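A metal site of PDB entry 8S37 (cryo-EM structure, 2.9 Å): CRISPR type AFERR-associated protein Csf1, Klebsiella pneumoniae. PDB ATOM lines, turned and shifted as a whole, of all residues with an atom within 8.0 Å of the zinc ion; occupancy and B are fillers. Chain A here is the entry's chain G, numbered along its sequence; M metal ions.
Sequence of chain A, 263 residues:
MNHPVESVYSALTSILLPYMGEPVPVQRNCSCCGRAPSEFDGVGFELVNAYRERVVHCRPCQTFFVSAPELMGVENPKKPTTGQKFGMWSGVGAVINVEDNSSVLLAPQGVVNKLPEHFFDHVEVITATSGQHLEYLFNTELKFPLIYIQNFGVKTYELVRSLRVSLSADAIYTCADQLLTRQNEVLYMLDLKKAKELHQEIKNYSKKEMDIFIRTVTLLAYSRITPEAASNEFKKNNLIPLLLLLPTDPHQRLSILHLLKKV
Merely in contact with the zinc ion: Arg 35 (3.1 Å).
The nearest printed residue that does not touch the zinc ion is Phe 40 (4.04 Å).
The side-chain sulfur (SG) of Cys 58 sits close to the guanidinium group (NH2) of Arg 35 (2.7 Å).
SG of Cys 30 sits close to N of Cys 32, 3.1 Å away.
The side-chain sulfur (SG) of Cys 30 sits close to the backbone carbonyl oxygen (O) of Val 56 (3.6 Å).
The side-chain sulfur of Cys 33 lies close to the guanidinium group of Arg 35 (2.7 Å).
The guanidinium group (NH1) of Arg 35 lies within salt-bridge range of the side-chain carboxylate (OE2) of Glu 39, at 2.8 Å.
The zinc ion is bound by the side-chain sulfur of Cys 58 (2.3 Å), the side-chain sulfur of Cys 30 (2.3 Å), the side-chain sulfur of Cys 33 (2.3 Å) and the side-chain sulfur of Cys 61 (2.3 Å).
The zinc ion has four donor atoms within binding distance.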
ATOM      1  N   VAL A   5     -11.963  -9.910 -16.161  1.00  0.00           N
ATOM      2  CA  VAL A   5     -13.226  -9.538 -15.526  1.00  0.00           C
ATOM      3  C   VAL A   5     -13.541  -8.075 -15.812  1.00  0.00           C
ATOM      4  O   VAL A   5     -14.714  -7.711 -15.990  1.00  0.00           O
ATOM      5  CB  VAL A   5     -13.172  -9.805 -14.019  1.00  0.00           C
ATOM      6  CG1 VAL A   5     -14.538  -9.564 -13.377  1.00  0.00           C
ATOM      7  CG2 VAL A   5     -12.691 -11.225 -13.738  1.00  0.00           C
ATOM      8  N   GLU A   6     -12.520  -7.232 -15.943  1.00  0.00           N
ATOM      9  CA  GLU A   6     -12.762  -5.875 -16.400  1.00  0.00           C
ATOM     10  C   GLU A   6     -13.318  -5.869 -17.813  1.00  0.00           C
ATOM     11  O   GLU A   6     -14.231  -5.098 -18.127  1.00  0.00           O
ATOM     12  CB  GLU A   6     -11.471  -5.063 -16.327  1.00  0.00           C
ATOM     13  CG  GLU A   6     -11.664  -3.562 -16.544  1.00  0.00           C
ATOM     14  CD  GLU A   6     -12.522  -2.916 -15.470  1.00  0.00           C
ATOM     15  OE1 GLU A   6     -12.677  -3.527 -14.394  1.00  0.00           O
ATOM     16  OE2 GLU A   6     -13.029  -1.805 -15.706  1.00  0.00           O
ATOM     17  N   ASN A  29      -7.977  -7.162  -0.959  1.00  0.00           N
ATOM     18  CA  ASN A  29      -8.197  -7.695  -2.307  1.00  0.00           C
ATOM     19  C   ASN A  29      -9.629  -8.200  -2.480  1.00  0.00           C
ATOM     20  O   ASN A  29     -10.243  -8.712  -1.547  1.00  0.00           O
ATOM     21  CB  ASN A  29      -7.219  -8.837  -2.590  1.00  0.00           C
ATOM     22  CG  ASN A  29      -7.208  -9.898  -1.511  1.00  0.00           C
ATOM     23  OD1 ASN A  29      -8.044  -9.885  -0.604  1.00  0.00           O
ATOM     24  ND2 ASN A  29      -6.269 -10.827  -1.594  1.00  0.00           N
ATOM     25  N   CYS A  30     -10.155  -8.009  -3.690  1.00  0.00           N
ATOM     26  CA  CYS A  30     -11.474  -8.523  -4.035  1.00  0.00           C
ATOM     27  C   CYS A  30     -11.558 -10.016  -3.780  1.00  0.00           C
ATOM     28  O   CYS A  30     -10.785 -10.791  -4.356  1.00  0.00           O
ATOM     29  CB  CYS A  30     -11.793  -8.220  -5.504  1.00  0.00           C
ATOM     30  SG  CYS A  30     -13.213  -9.152  -6.140  1.00  0.00           S
ATOM     31  N   SER A  31     -12.503 -10.413  -2.933  1.00  0.00           N
ATOM     32  CA  SER A  31     -12.707 -11.824  -2.634  1.00  0.00           C
ATOM     33  C   SER A  31     -13.209 -12.611  -3.830  1.00  0.00           C
ATOM     34  O   SER A  31     -13.168 -13.842  -3.792  1.00  0.00           O
ATOM     35  CB  SER A  31     -13.684 -11.961  -1.466  1.00  0.00           C
ATOM     36  OG  SER A  31     -14.913 -11.339  -1.763  1.00  0.00           O
ATOM     37  N   CYS A  32     -13.682 -11.946  -4.883  1.00  0.00           N
ATOM     38  CA  CYS A  32     -14.299 -12.642  -6.005  1.00  0.00           C
ATOM     39  C   CYS A  32     -13.271 -12.994  -7.079  1.00  0.00           C
ATOM     40  O   CYS A  32     -13.110 -14.172  -7.413  1.00  0.00           O
ATOM     41  CB  CYS A  32     -15.411 -11.756  -6.599  1.00  0.00           C
ATOM     42  SG  CYS A  32     -16.719 -12.646  -7.466  1.00  0.00           S
ATOM     43  N   CYS A  33     -12.567 -11.993  -7.607  1.00  0.00           N
ATOM     44  CA  CYS A  33     -11.501 -12.290  -8.563  1.00  0.00           C
ATOM     45  C   CYS A  33     -10.194 -12.655  -7.855  1.00  0.00           C
ATOM     46  O   CYS A  33      -9.439 -13.499  -8.341  1.00  0.00           O
ATOM     47  CB  CYS A  33     -11.263 -11.106  -9.493  1.00  0.00           C
ATOM     48  SG  CYS A  33     -10.834  -9.593  -8.656  1.00  0.00           S
ATOM     49  N   GLY A  34      -9.925 -12.034  -6.711  1.00  0.00           N
ATOM     50  CA  GLY A  34      -8.703 -12.259  -5.982  1.00  0.00           C
ATOM     51  C   GLY A  34      -7.571 -11.315  -6.322  1.00  0.00           C
ATOM     52  O   GLY A  34      -6.522 -11.370  -5.673  1.00  0.00           O
ATOM     53  N   ARG A  35      -7.752 -10.429  -7.299  1.00  0.00           N
ATOM     54  CA  ARG A  35      -6.680  -9.528  -7.695  1.00  0.00           C
ATOM     55  C   ARG A  35      -6.396  -8.536  -6.564  1.00  0.00           C
ATOM     56  O   ARG A  35      -7.164  -8.390  -5.610  1.00  0.00           O
ATOM     57  CB  ARG A  35      -7.056  -8.779  -8.967  1.00  0.00           C
ATOM     58  CG  ARG A  35      -7.397  -9.673 -10.161  1.00  0.00           C
ATOM     59  CD  ARG A  35      -8.186  -8.925 -11.221  1.00  0.00           C
ATOM     60  NE  ARG A  35      -9.497  -8.506 -10.721  1.00  0.00           N
ATOM     61  CZ  ARG A  35     -10.358  -7.755 -11.393  1.00  0.00           C
ATOM     62  NH1 ARG A  35     -10.091  -7.304 -12.605  1.00  0.00           N
ATOM     63  NH2 ARG A  35     -11.524  -7.452 -10.840  1.00  0.00           N
ATOM     64  N   ALA A  36      -5.296  -7.802  -6.705  1.00  0.00           N
ATOM     65  CA  ALA A  36      -4.906  -6.871  -5.666  1.00  0.00           C
ATOM     66  C   ALA A  36      -5.696  -5.572  -5.789  1.00  0.00           C
ATOM     67  O   ALA A  36      -6.165  -5.228  -6.881  1.00  0.00           O
ATOM     68  CB  ALA A  36      -3.410  -6.580  -5.746  1.00  0.00           C
ATOM     69  N   GLU A  39      -4.985  -2.390  -8.649  1.00  0.00           N
ATOM     70  CA  GLU A  39      -5.615  -2.147  -9.929  1.00  0.00           C
ATOM     71  C   GLU A  39      -7.105  -1.816  -9.815  1.00  0.00           C
ATOM     72  O   GLU A  39      -7.754  -1.615 -10.842  1.00  0.00           O
ATOM     73  CB  GLU A  39      -5.425  -3.361 -10.840  1.00  0.00           C
ATOM     74  CG  GLU A  39      -6.269  -4.586 -10.474  1.00  0.00           C
ATOM     75  CD  GLU A  39      -7.539  -4.737 -11.298  1.00  0.00           C
ATOM     76  OE1 GLU A  39      -7.830  -3.872 -12.154  1.00  0.00           O
ATOM     77  OE2 GLU A  39      -8.247  -5.743 -11.101  1.00  0.00           O
ATOM     78  N   PHE A  40      -7.640  -1.727  -8.594  1.00  0.00           N
ATOM     79  CA  PHE A  40      -8.980  -1.191  -8.390  1.00  0.00           C
ATOM     80  C   PHE A  40      -8.977   0.314  -8.164  1.00  0.00           C
ATOM     81  O   PHE A  40     -10.034   0.891  -7.906  1.00  0.00           O
ATOM     82  CB  PHE A  40      -9.655  -1.872  -7.184  1.00  0.00           C
ATOM     83  CG  PHE A  40      -9.767  -3.366  -7.308  1.00  0.00           C
ATOM     84  CD1 PHE A  40      -9.773  -4.003  -8.539  1.00  0.00           C
ATOM     85  CD2 PHE A  40      -9.903  -4.142  -6.167  1.00  0.00           C
ATOM     86  CE1 PHE A  40      -9.880  -5.378  -8.621  1.00  0.00           C
ATOM     87  CE2 PHE A  40      -9.998  -5.508  -6.250  1.00  0.00           C
ATOM     88  CZ  PHE A  40     -10.003  -6.135  -7.480  1.00  0.00           C
ATOM     89  N   VAL A  56     -15.530  -8.149  -0.241  1.00  0.00           N
ATOM     90  CA  VAL A  56     -15.309  -7.044  -1.162  1.00  0.00           C
ATOM     91  C   VAL A  56     -15.335  -7.585  -2.589  1.00  0.00           C
ATOM     92  O   VAL A  56     -14.646  -8.556  -2.900  1.00  0.00           O
ATOM     93  CB  VAL A  56     -13.983  -6.319  -0.863  1.00  0.00           C
ATOM     94  CG1 VAL A  56     -12.797  -7.274  -0.861  1.00  0.00           C
ATOM     95  CG2 VAL A  56     -13.768  -5.191  -1.863  1.00  0.00           C
ATOM     96  N   HIS A  57     -16.144  -6.958  -3.430  1.00  0.00           N
ATOM     97  CA  HIS A  57     -16.142  -7.201  -4.873  1.00  0.00           C
ATOM     98  C   HIS A  57     -15.795  -5.890  -5.550  1.00  0.00           C
ATOM     99  O   HIS A  57     -16.196  -4.820  -5.093  1.00  0.00           O
ATOM    100  CB  HIS A  57     -17.494  -7.709  -5.355  1.00  0.00           C
ATOM    101  CG  HIS A  57     -17.957  -8.958  -4.686  1.00  0.00           C
ATOM    102  ND1 HIS A  57     -19.266  -9.387  -4.718  1.00  0.00           N
ATOM    103  CD2 HIS A  57     -17.279  -9.881  -3.949  1.00  0.00           C
ATOM    104  CE1 HIS A  57     -19.373 -10.521  -4.040  1.00  0.00           C
ATOM    105  NE2 HIS A  57     -18.186 -10.839  -3.571  1.00  0.00           N
ATOM    106  N   CYS A  58     -15.066  -5.970  -6.658  1.00  0.00           N
ATOM    107  CA  CYS A  58     -14.658  -4.756  -7.343  1.00  0.00           C
ATOM    108  C   CYS A  58     -15.705  -4.374  -8.388  1.00  0.00           C
ATOM    109  O   CYS A  58     -16.654  -5.118  -8.643  1.00  0.00           O
ATOM    110  CB  CYS A  58     -13.279  -4.948  -7.996  1.00  0.00           C
ATOM    111  SG  CYS A  58     -13.102  -6.462  -8.943  1.00  0.00           S
ATOM    112  N   ARG A  59     -15.530  -3.177  -8.960  1.00  0.00           N
ATOM    113  CA  ARG A  59     -16.431  -2.659  -9.995  1.00  0.00           C
ATOM    114  C   ARG A  59     -16.842  -3.710 -11.024  1.00  0.00           C
ATOM    115  O   ARG A  59     -18.042  -3.876 -11.242  1.00  0.00           O
ATOM    116  CB  ARG A  59     -15.741  -1.464 -10.668  1.00  0.00           C
ATOM    117  CG  ARG A  59     -16.429  -0.925 -11.925  1.00  0.00           C
ATOM    118  CD  ARG A  59     -17.881  -0.549 -11.673  1.00  0.00           C
ATOM    119  NE  ARG A  59     -18.017   0.446 -10.611  1.00  0.00           N
ATOM    120  CZ  ARG A  59     -17.759   1.739 -10.747  1.00  0.00           C
ATOM    121  NH1 ARG A  59     -17.358   2.256 -11.900  1.00  0.00           N
ATOM    122  NH2 ARG A  59     -17.916   2.545  -9.698  1.00  0.00           N
ATOM    123  N   PRO A  60     -15.930  -4.438 -11.674  1.00  0.00           N
ATOM    124  CA  PRO A  60     -16.371  -5.476 -12.609  1.00  0.00           C
ATOM    125  C   PRO A  60     -16.961  -6.691 -11.927  1.00  0.00           C
ATOM    126  O   PRO A  60     -17.876  -7.314 -12.475  1.00  0.00           O
ATOM    127  CB  PRO A  60     -15.088  -5.808 -13.376  1.00  0.00           C
ATOM    128  CG  PRO A  60     -14.026  -5.578 -12.390  1.00  0.00           C
ATOM    129  CD  PRO A  60     -14.453  -4.358 -11.626  1.00  0.00           C
ATOM    130  N   CYS A  61     -16.464  -7.059 -10.738  1.00  0.00           N
ATOM    131  CA  CYS A  61     -16.946  -8.276 -10.086  1.00  0.00           C
ATOM    132  C   CYS A  61     -18.291  -8.056  -9.426  1.00  0.00           C
ATOM    133  O   CYS A  61     -19.140  -8.955  -9.434  1.00  0.00           O
ATOM    134  CB  CYS A  61     -15.920  -8.756  -9.052  1.00  0.00           C
ATOM    135  SG  CYS A  61     -14.584  -9.748  -9.729  1.00  0.00           S
ATOM    136  N   GLN A  62     -18.519  -6.874  -8.853  1.00  0.00           N
ATOM    137  CA  GLN A  62     -19.789  -6.623  -8.180  1.00  0.00           C
ATOM    138  C   GLN A  62     -20.954  -6.591  -9.151  1.00  0.00           C
ATOM    139  O   GLN A  62     -22.106  -6.721  -8.719  1.00  0.00           O
ATOM    140  CB  GLN A  62     -19.710  -5.294  -7.413  1.00  0.00           C
ATOM    141  CG  GLN A  62     -21.011  -4.848  -6.742  1.00  0.00           C
ATOM    142  CD  GLN A  62     -21.608  -5.925  -5.865  1.00  0.00           C
ATOM    143  OE1 GLN A  62     -20.899  -6.759  -5.310  1.00  0.00           O
ATOM    144  NE2 GLN A  62     -22.927  -5.913  -5.735  1.00  0.00           N
ATOM    145  N   PHE A  65     -23.484  -9.522  -8.971  1.00  0.00           N
ATOM    146  CA  PHE A  65     -24.332  -9.692  -7.786  1.00  0.00           C
ATOM    147  C   PHE A  65     -25.406  -8.619  -7.686  1.00  0.00           C
ATOM    148  O   PHE A  65     -25.906  -8.361  -6.595  1.00  0.00           O
ATOM    149  CB  PHE A  65     -23.469  -9.707  -6.524  1.00  0.00           C
ATOM    150  CG  PHE A  65     -22.373 -10.723  -6.555  1.00  0.00           C
ATOM    151  CD1 PHE A  65     -21.150 -10.439  -7.131  1.00  0.00           C
ATOM    152  CD2 PHE A  65     -22.564 -11.978  -5.993  1.00  0.00           C
ATOM    153  CE1 PHE A  65     -20.145 -11.375  -7.151  1.00  0.00           C
ATOM    154  CE2 PHE A  65     -21.561 -12.925  -6.013  1.00  0.00           C
ATOM    155  CZ  PHE A  65     -20.346 -12.619  -6.597  1.00  0.00           C
ATOM    156  N   VAL A 160     -15.309 -15.763 -12.220  1.00  0.00           N
ATOM    157  CA  VAL A 160     -14.485 -14.588 -12.434  1.00  0.00           C
ATOM    158  C   VAL A 160     -13.003 -14.951 -12.397  1.00  0.00           C
ATOM    159  O   VAL A 160     -12.222 -14.487 -13.237  1.00  0.00           O
ATOM    160  CB  VAL A 160     -14.826 -13.471 -11.420  1.00  0.00           C
ATOM    161  CG1 VAL A 160     -16.263 -13.030 -11.590  1.00  0.00           C
ATOM    162  CG2 VAL A 160     -14.555 -13.910  -9.989  1.00  0.00           C
ATOM    163  N   ARG A 161     -12.589 -15.800 -11.443  1.00  0.00           N
ATOM    164  CA  ARG A 161     -11.169 -16.167 -11.420  1.00  0.00           C
ATOM    165  C   ARG A 161     -10.845 -17.272 -12.412  1.00  0.00           C
ATOM    166  O   ARG A 161      -9.671 -17.673 -12.496  1.00  0.00           O
ATOM    167  CB  ARG A 161     -10.731 -16.552  -9.994  1.00  0.00           C
ATOM    168  CG  ARG A 161     -11.129 -17.916  -9.464  1.00  0.00           C
ATOM    169  CD  ARG A 161     -10.544 -18.115  -8.069  1.00  0.00           C
ATOM    170  NE  ARG A 161     -11.055 -17.151  -7.092  1.00  0.00           N
ATOM    171  CZ  ARG A 161     -12.052 -17.362  -6.245  1.00  0.00           C
ATOM    172  NH1 ARG A 161     -12.711 -18.511  -6.217  1.00  0.00           N
ATOM    173  NH2 ARG A 161     -12.396 -16.403  -5.405  1.00  0.00           N
HETATM  174 ZN    ZN M   1     -12.973  -8.714  -8.405  1.00  0.00          ZN
